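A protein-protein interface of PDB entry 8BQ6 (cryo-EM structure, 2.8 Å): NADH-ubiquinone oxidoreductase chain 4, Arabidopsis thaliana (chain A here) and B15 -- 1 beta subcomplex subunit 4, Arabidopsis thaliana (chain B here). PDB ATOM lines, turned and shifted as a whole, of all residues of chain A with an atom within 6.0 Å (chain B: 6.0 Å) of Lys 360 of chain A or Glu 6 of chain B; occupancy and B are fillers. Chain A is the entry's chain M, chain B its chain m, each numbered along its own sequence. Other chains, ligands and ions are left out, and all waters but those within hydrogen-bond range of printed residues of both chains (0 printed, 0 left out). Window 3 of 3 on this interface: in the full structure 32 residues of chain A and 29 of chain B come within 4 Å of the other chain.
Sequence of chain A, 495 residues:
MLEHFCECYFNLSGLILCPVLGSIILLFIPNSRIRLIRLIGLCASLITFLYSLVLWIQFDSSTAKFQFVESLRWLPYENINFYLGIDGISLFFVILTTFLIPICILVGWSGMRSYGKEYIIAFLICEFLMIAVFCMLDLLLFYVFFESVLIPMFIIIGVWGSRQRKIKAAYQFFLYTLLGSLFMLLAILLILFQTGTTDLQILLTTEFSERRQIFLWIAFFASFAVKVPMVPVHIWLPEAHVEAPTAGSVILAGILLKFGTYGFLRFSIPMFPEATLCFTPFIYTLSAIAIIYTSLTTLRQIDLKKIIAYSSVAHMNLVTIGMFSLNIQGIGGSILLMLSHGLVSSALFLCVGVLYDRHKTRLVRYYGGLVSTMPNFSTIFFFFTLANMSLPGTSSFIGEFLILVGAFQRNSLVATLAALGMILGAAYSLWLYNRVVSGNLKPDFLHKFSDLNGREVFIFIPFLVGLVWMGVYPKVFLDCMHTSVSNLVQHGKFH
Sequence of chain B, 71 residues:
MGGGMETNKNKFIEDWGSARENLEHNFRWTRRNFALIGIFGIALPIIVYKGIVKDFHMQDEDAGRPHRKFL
Printed residues of chain B within 4 Å of Lys 360 of chain A: Glu 6 (3.3 Å), Thr 7 (3.99 Å) and Lys 9 (3.98 Å). Of chain A, only Arg 358 (3.9 Å), His 359 (3.5 Å) and Lys 360 (3.3 Å) come within 4 Å of Glu 6 of chain B. Of the printed residues of chain A, Thr 7 of chain B touches His 359 (3.0 Å), Lys 360 (3.99 Å), Thr 361 (3.6 Å), Phe 445 (3.3 Å) and Leu 446 (3.7 Å). Of the printed residues of chain B, Arg 358 of chain A touches Met 5 and Glu 6.
O of Arg 358 of chain A touches CB of Met 5 of chain B (3.5 Å). Glu 6 of chain B touches Arg 358 of chain A (N to O, 3.9 Å). His 359 of chain A touches Glu 6 of chain B (O to CA, 3.5 Å). CG2 of Thr 7 of chain B touches O of Lys 360 of chain A (3.99 Å). Lys 360 of chain A touches Lys 9 of chain B. Thr 361 of chain A touches Thr 7 of chain B (CB to CG2, 3.6 Å). CD2 of Leu 446 of chain A touches O of Met 5 of chain B, 3.5 Å away. CA of Thr 7 of chain B touches CD2 of Leu 446 of chain A, 3.7 Å away.
A ring nitrogen (ND1) of His 359 of chain A is in hydrogen-bond range of the backbone carbonyl oxygen of Met 5 of chain B (3.1 Å). O of His 359 of chain A sits at hydrogen-bond distance from N of Thr 7 of chain B (3.0 Å). OE2 of Glu 6 of chain B is in salt-bridge range of NZ of Lys 360 of chain A (3.3 Å). The side-chain hydroxyl (OG1) of Thr 7 of chain B lies close to the backbone carbonyl oxygen (O) of Phe 445 of chain A. O of Phe 445 of chain A sits at hydrogen-bond distance from N of Asn 8 of chain B, 3.0 Å away.
Of the 13 printed residues of chain A, 6 touch a printed residue of chain B. Hydrophobic or aromatic side chains of chain A within 4 Å of the printed part of chain B: His 359, Phe 445 and Leu 446. Of the 7 printed residues of chain B, 5 touch a printed residue of chain A. Hydrophobic or aromatic side chains of chain B that line the printed part of chain A: Met 5.
NZ of Lys 360 of chain A is in hydrogen-bond range of O of Asp 357 of chain A, at 3.3 Å. O of Thr 361 of chain A lies within hydrogen-bond range of OH of Tyr 367 of chain A (2.7 Å).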
ATOM      1  N   SER A 162      19.747  -3.729  -3.263  1.00  0.00           N
ATOM      2  CA  SER A 162      19.358  -2.843  -2.170  1.00  0.00           C
ATOM      3  C   SER A 162      19.123  -3.585  -0.858  1.00  0.00           C
ATOM      4  O   SER A 162      19.395  -3.040   0.216  1.00  0.00           O
ATOM      5  CB  SER A 162      18.107  -2.060  -2.556  1.00  0.00           C
ATOM      6  OG  SER A 162      17.682  -1.226  -1.493  1.00  0.00           O
ATOM      7  N   LEU A 355      12.630   7.229  -8.360  1.00  0.00           N
ATOM      8  CA  LEU A 355      11.823   7.291  -7.146  1.00  0.00           C
ATOM      9  C   LEU A 355      12.506   6.590  -5.979  1.00  0.00           C
ATOM     10  O   LEU A 355      12.369   7.014  -4.826  1.00  0.00           O
ATOM     11  CB  LEU A 355      10.458   6.657  -7.392  1.00  0.00           C
ATOM     12  CG  LEU A 355       9.388   7.446  -8.139  1.00  0.00           C
ATOM     13  CD1 LEU A 355       8.047   6.793  -7.901  1.00  0.00           C
ATOM     14  CD2 LEU A 355       9.370   8.895  -7.699  1.00  0.00           C
ATOM     15  N   TYR A 356      13.207   5.489  -6.252  1.00  0.00           N
ATOM     16  CA  TYR A 356      13.766   4.685  -5.172  1.00  0.00           C
ATOM     17  C   TYR A 356      15.014   5.325  -4.577  1.00  0.00           C
ATOM     18  O   TYR A 356      15.238   5.243  -3.363  1.00  0.00           O
ATOM     19  CB  TYR A 356      14.085   3.282  -5.674  1.00  0.00           C
ATOM     20  CG  TYR A 356      14.492   2.353  -4.568  1.00  0.00           C
ATOM     21  CD1 TYR A 356      13.544   1.722  -3.778  1.00  0.00           C
ATOM     22  CD2 TYR A 356      15.830   2.137  -4.286  1.00  0.00           C
ATOM     23  CE1 TYR A 356      13.922   0.880  -2.758  1.00  0.00           C
ATOM     24  CE2 TYR A 356      16.215   1.305  -3.271  1.00  0.00           C
ATOM     25  CZ  TYR A 356      15.261   0.679  -2.508  1.00  0.00           C
ATOM     26  OH  TYR A 356      15.658  -0.154  -1.492  1.00  0.00           O
ATOM     27  N   ASP A 357      15.849   5.944  -5.414  1.00  0.00           N
ATOM     28  CA  ASP A 357      17.067   6.572  -4.911  1.00  0.00           C
ATOM     29  C   ASP A 357      16.760   7.664  -3.899  1.00  0.00           C
ATOM     30  O   ASP A 357      17.545   7.887  -2.970  1.00  0.00           O
ATOM     31  CB  ASP A 357      17.882   7.151  -6.066  1.00  0.00           C
ATOM     32  CG  ASP A 357      18.382   6.089  -7.014  1.00  0.00           C
ATOM     33  OD1 ASP A 357      19.090   6.444  -7.979  1.00  0.00           O
ATOM     34  OD2 ASP A 357      18.068   4.901  -6.795  1.00  0.00           O
ATOM     35  N   ARG A 358      15.633   8.354  -4.060  1.00  0.00           N
ATOM     36  CA  ARG A 358      15.254   9.419  -3.142  1.00  0.00           C
ATOM     37  C   ARG A 358      14.562   8.892  -1.892  1.00  0.00           C
ATOM     38  O   ARG A 358      14.948   9.244  -0.773  1.00  0.00           O
ATOM     39  CB  ARG A 358      14.340  10.428  -3.839  1.00  0.00           C
ATOM     40  CG  ARG A 358      14.987  11.191  -4.962  1.00  0.00           C
ATOM     41  CD  ARG A 358      13.949  11.601  -5.974  1.00  0.00           C
ATOM     42  NE  ARG A 358      14.436  12.653  -6.854  1.00  0.00           N
ATOM     43  CZ  ARG A 358      15.302  12.463  -7.837  1.00  0.00           C
ATOM     44  NH1 ARG A 358      15.800  11.264  -8.097  1.00  0.00           N
ATOM     45  NH2 ARG A 358      15.678  13.499  -8.579  1.00  0.00           N
ATOM     46  N   HIS A 359      13.486   8.122  -2.086  1.00  0.00           N
ATOM     47  CA  HIS A 359      12.616   7.721  -0.945  1.00  0.00           C
ATOM     48  C   HIS A 359      12.854   6.304  -0.417  1.00  0.00           C
ATOM     49  O   HIS A 359      12.308   6.017   0.658  1.00  0.00           O
ATOM     50  CB  HIS A 359      11.161   7.923  -1.372  1.00  0.00           C
ATOM     51  CG  HIS A 359      10.918   9.204  -2.100  1.00  0.00           C
ATOM     52  ND1 HIS A 359      11.162  10.437  -1.528  1.00  0.00           N
ATOM     53  CD2 HIS A 359      10.461   9.452  -3.345  1.00  0.00           C
ATOM     54  CE1 HIS A 359      10.857  11.387  -2.386  1.00  0.00           C
ATOM     55  NE2 HIS A 359      10.429  10.810  -3.509  1.00  0.00           N
ATOM     56  N   LYS A 360      13.567   5.440  -1.139  1.00  0.00           N
ATOM     57  CA  LYS A 360      13.925   4.108  -0.651  1.00  0.00           C
ATOM     58  C   LYS A 360      12.692   3.270  -0.315  1.00  0.00           C
ATOM     59  O   LYS A 360      12.566   2.715   0.778  1.00  0.00           O
ATOM     60  CB  LYS A 360      14.855   4.207   0.558  1.00  0.00           C
ATOM     61  CG  LYS A 360      16.134   4.959   0.287  1.00  0.00           C
ATOM     62  CD  LYS A 360      17.128   4.069  -0.427  1.00  0.00           C
ATOM     63  CE  LYS A 360      18.498   4.711  -0.469  1.00  0.00           C
ATOM     64  NZ  LYS A 360      18.402   6.181  -0.279  1.00  0.00           N
ATOM     65  N   THR A 361      11.777   3.171  -1.275  1.00  0.00           N
ATOM     66  CA  THR A 361      10.670   2.236  -1.152  1.00  0.00           C
ATOM     67  C   THR A 361      10.121   1.936  -2.537  1.00  0.00           C
ATOM     68  O   THR A 361      10.147   2.786  -3.431  1.00  0.00           O
ATOM     69  CB  THR A 361       9.553   2.764  -0.243  1.00  0.00           C
ATOM     70  OG1 THR A 361       8.597   1.723  -0.020  1.00  0.00           O
ATOM     71  CG2 THR A 361       8.850   3.951  -0.879  1.00  0.00           C
ATOM     72  N   ARG A 362       9.644   0.707  -2.708  1.00  0.00           N
ATOM     73  CA  ARG A 362       9.044   0.274  -3.959  1.00  0.00           C
ATOM     74  C   ARG A 362       7.548   0.021  -3.840  1.00  0.00           C
ATOM     75  O   ARG A 362       6.914  -0.340  -4.836  1.00  0.00           O
ATOM     76  CB  ARG A 362       9.743  -0.990  -4.471  1.00  0.00           C
ATOM     77  CG  ARG A 362      11.148  -0.759  -4.993  1.00  0.00           C
ATOM     78  CD  ARG A 362      11.617  -1.932  -5.838  1.00  0.00           C
ATOM     79  NE  ARG A 362      11.675  -3.182  -5.090  1.00  0.00           N
ATOM     80  CZ  ARG A 362      12.699  -3.556  -4.333  1.00  0.00           C
ATOM     81  NH1 ARG A 362      13.773  -2.798  -4.202  1.00  0.00           N
ATOM     82  NH2 ARG A 362      12.643  -4.722  -3.697  1.00  0.00           N
ATOM     83  N   TYR A 367       3.408   6.031  -2.288  1.00  0.00           N
ATOM     84  CA  TYR A 367       3.484   7.115  -3.250  1.00  0.00           C
ATOM     85  C   TYR A 367       2.089   7.659  -3.542  1.00  0.00           C
ATOM     86  O   TYR A 367       1.108   7.333  -2.870  1.00  0.00           O
ATOM     87  CB  TYR A 367       4.173   6.641  -4.528  1.00  0.00           C
ATOM     88  CG  TYR A 367       5.640   6.321  -4.357  1.00  0.00           C
ATOM     89  CD1 TYR A 367       6.581   7.327  -4.190  1.00  0.00           C
ATOM     90  CD2 TYR A 367       6.081   5.008  -4.359  1.00  0.00           C
ATOM     91  CE1 TYR A 367       7.921   7.029  -4.034  1.00  0.00           C
ATOM     92  CE2 TYR A 367       7.413   4.703  -4.203  1.00  0.00           C
ATOM     93  CZ  TYR A 367       8.328   5.714  -4.041  1.00  0.00           C
ATOM     94  OH  TYR A 367       9.655   5.395  -3.887  1.00  0.00           O
ATOM     95  N   PHE A 445       3.915   9.730   5.007  1.00  0.00           N
ATOM     96  CA  PHE A 445       4.925   8.852   4.431  1.00  0.00           C
ATOM     97  C   PHE A 445       6.053   9.624   3.762  1.00  0.00           C
ATOM     98  O   PHE A 445       7.230   9.348   4.013  1.00  0.00           O
ATOM     99  CB  PHE A 445       4.295   7.901   3.410  1.00  0.00           C
ATOM    100  CG  PHE A 445       3.107   7.158   3.925  1.00  0.00           C
ATOM    101  CD1 PHE A 445       3.110   6.624   5.198  1.00  0.00           C
ATOM    102  CD2 PHE A 445       1.996   6.970   3.124  1.00  0.00           C
ATOM    103  CE1 PHE A 445       2.022   5.934   5.669  1.00  0.00           C
ATOM    104  CE2 PHE A 445       0.907   6.278   3.590  1.00  0.00           C
ATOM    105  CZ  PHE A 445       0.919   5.761   4.864  1.00  0.00           C
ATOM    106  N   LEU A 446       5.690  10.604   2.934  1.00  0.00           N
ATOM    107  CA  LEU A 446       6.701  11.374   2.170  1.00  0.00           C
ATOM    108  C   LEU A 446       6.343  12.856   2.222  1.00  0.00           C
ATOM    109  O   LEU A 446       5.188  13.188   1.896  1.00  0.00           O
ATOM    110  CB  LEU A 446       6.674  10.870   0.726  1.00  0.00           C
ATOM    111  CG  LEU A 446       7.391   9.546   0.485  1.00  0.00           C
ATOM    112  CD1 LEU A 446       7.256   9.110  -0.962  1.00  0.00           C
ATOM    113  CD2 LEU A 446       8.848   9.674   0.876  1.00  0.00           C
ATOM    114  N   HIS A 447       7.300  13.714   2.560  1.00  0.00           N
ATOM    115  CA  HIS A 447       7.021  15.168   2.693  1.00  0.00           C
ATOM    116  C   HIS A 447       8.132  15.990   2.033  1.00  0.00           C
ATOM    117  O   HIS A 447       7.910  17.178   1.819  1.00  0.00           O
ATOM    118  CB  HIS A 447       6.830  15.536   4.172  1.00  0.00           C
ATOM    119  CG  HIS A 447       7.973  15.138   5.043  1.00  0.00           C
ATOM    120  ND1 HIS A 447       9.060  15.959   5.255  1.00  0.00           N
ATOM    121  CD2 HIS A 447       8.206  14.012   5.752  1.00  0.00           C
ATOM    122  CE1 HIS A 447       9.914  15.360   6.057  1.00  0.00           C
ATOM    123  NE2 HIS A 447       9.414  14.164   6.377  1.00  0.00           N
ATOM    124  N   GLY B   3      13.182  14.796   9.088  1.00  0.00           N
ATOM    125  CA  GLY B   3      14.528  14.663   8.571  1.00  0.00           C
ATOM    126  C   GLY B   3      14.694  13.632   7.477  1.00  0.00           C
ATOM    127  O   GLY B   3      14.434  12.442   7.683  1.00  0.00           O
ATOM    128  N   GLY B   4      15.152  14.086   6.311  1.00  0.00           N
ATOM    129  CA  GLY B   4      15.461  13.127   5.235  1.00  0.00           C
ATOM    130  C   GLY B   4      14.359  12.964   4.212  1.00  0.00           C
ATOM    131  O   GLY B   4      13.203  13.313   4.510  1.00  0.00           O
ATOM    132  N   MET B   5      14.719  12.430   3.042  1.00  0.00           N
ATOM    133  CA  MET B   5      13.715  12.170   1.985  1.00  0.00           C
ATOM    134  C   MET B   5      13.175  10.739   2.099  1.00  0.00           C
ATOM    135  O   MET B   5      12.167  10.471   1.439  1.00  0.00           O
ATOM    136  CB  MET B   5      14.340  12.371   0.604  1.00  0.00           C
ATOM    137  CG  MET B   5      14.602  13.822   0.265  1.00  0.00           C
ATOM    138  SD  MET B   5      15.231  14.015  -1.417  1.00  0.00           S
ATOM    139  CE  MET B   5      13.718  13.788  -2.345  1.00  0.00           C
ATOM    140  N   GLU B   6      13.803   9.855   2.890  1.00  0.00           N
ATOM    141  CA  GLU B   6      13.337   8.475   2.924  1.00  0.00           C
ATOM    142  C   GLU B   6      11.940   8.391   3.526  1.00  0.00           C
ATOM    143  O   GLU B   6      11.557   9.189   4.385  1.00  0.00           O
ATOM    144  CB  GLU B   6      14.314   7.601   3.714  1.00  0.00           C
ATOM    145  CG  GLU B   6      15.767   7.842   3.345  1.00  0.00           C
ATOM    146  CD  GLU B   6      16.648   6.613   3.514  1.00  0.00           C
ATOM    147  OE1 GLU B   6      16.254   5.677   4.241  1.00  0.00           O
ATOM    148  OE2 GLU B   6      17.743   6.590   2.917  1.00  0.00           O
ATOM    149  N   THR B   7      11.169   7.417   3.051  1.00  0.00           N
ATOM    150  CA  THR B   7       9.793   7.272   3.497  1.00  0.00           C
ATOM    151  C   THR B   7       9.742   6.874   4.965  1.00  0.00           C
ATOM    152  O   THR B   7      10.583   6.114   5.452  1.00  0.00           O
ATOM    153  CB  THR B   7       9.057   6.231   2.649  1.00  0.00           C
ATOM    154  OG1 THR B   7       7.755   5.994   3.199  1.00  0.00           O
ATOM    155  CG2 THR B   7       9.814   4.930   2.639  1.00  0.00           C
ATOM    156  N   ASN B   8       8.754   7.409   5.672  1.00  0.00           N
ATOM    157  CA  ASN B   8       8.485   7.007   7.044  1.00  0.00           C
ATOM    158  C   ASN B   8       7.743   5.681   7.015  1.00  0.00           C
ATOM    159  O   ASN B   8       6.555   5.630   6.680  1.00  0.00           O
ATOM    160  CB  ASN B   8       7.691   8.084   7.771  1.00  0.00           C
ATOM    161  CG  ASN B   8       8.585   9.081   8.459  1.00  0.00           C
ATOM    162  OD1 ASN B   8       9.022  10.061   7.858  1.00  0.00           O
ATOM    163  ND2 ASN B   8       8.887   8.824   9.724  1.00  0.00           N
ATOM    164  N   LYS B   9       8.453   4.610   7.352  1.00  0.00           N
ATOM    165  CA  LYS B   9       7.914   3.268   7.208  1.00  0.00           C
ATOM    166  C   LYS B   9       6.722   3.057   8.127  1.00  0.00           C
ATOM    167  O   LYS B   9       6.716   3.491   9.283  1.00  0.00           O
ATOM    168  CB  LYS B   9       8.990   2.234   7.526  1.00  0.00           C
ATOM    169  CG  LYS B   9       9.519   1.479   6.332  1.00  0.00           C
ATOM    170  CD  LYS B   9      10.226   2.385   5.347  1.00  0.00           C
ATOM    171  CE  LYS B   9      11.412   1.667   4.723  1.00  0.00           C
ATOM    172  NZ  LYS B   9      10.996   0.608   3.761  1.00  0.00           N
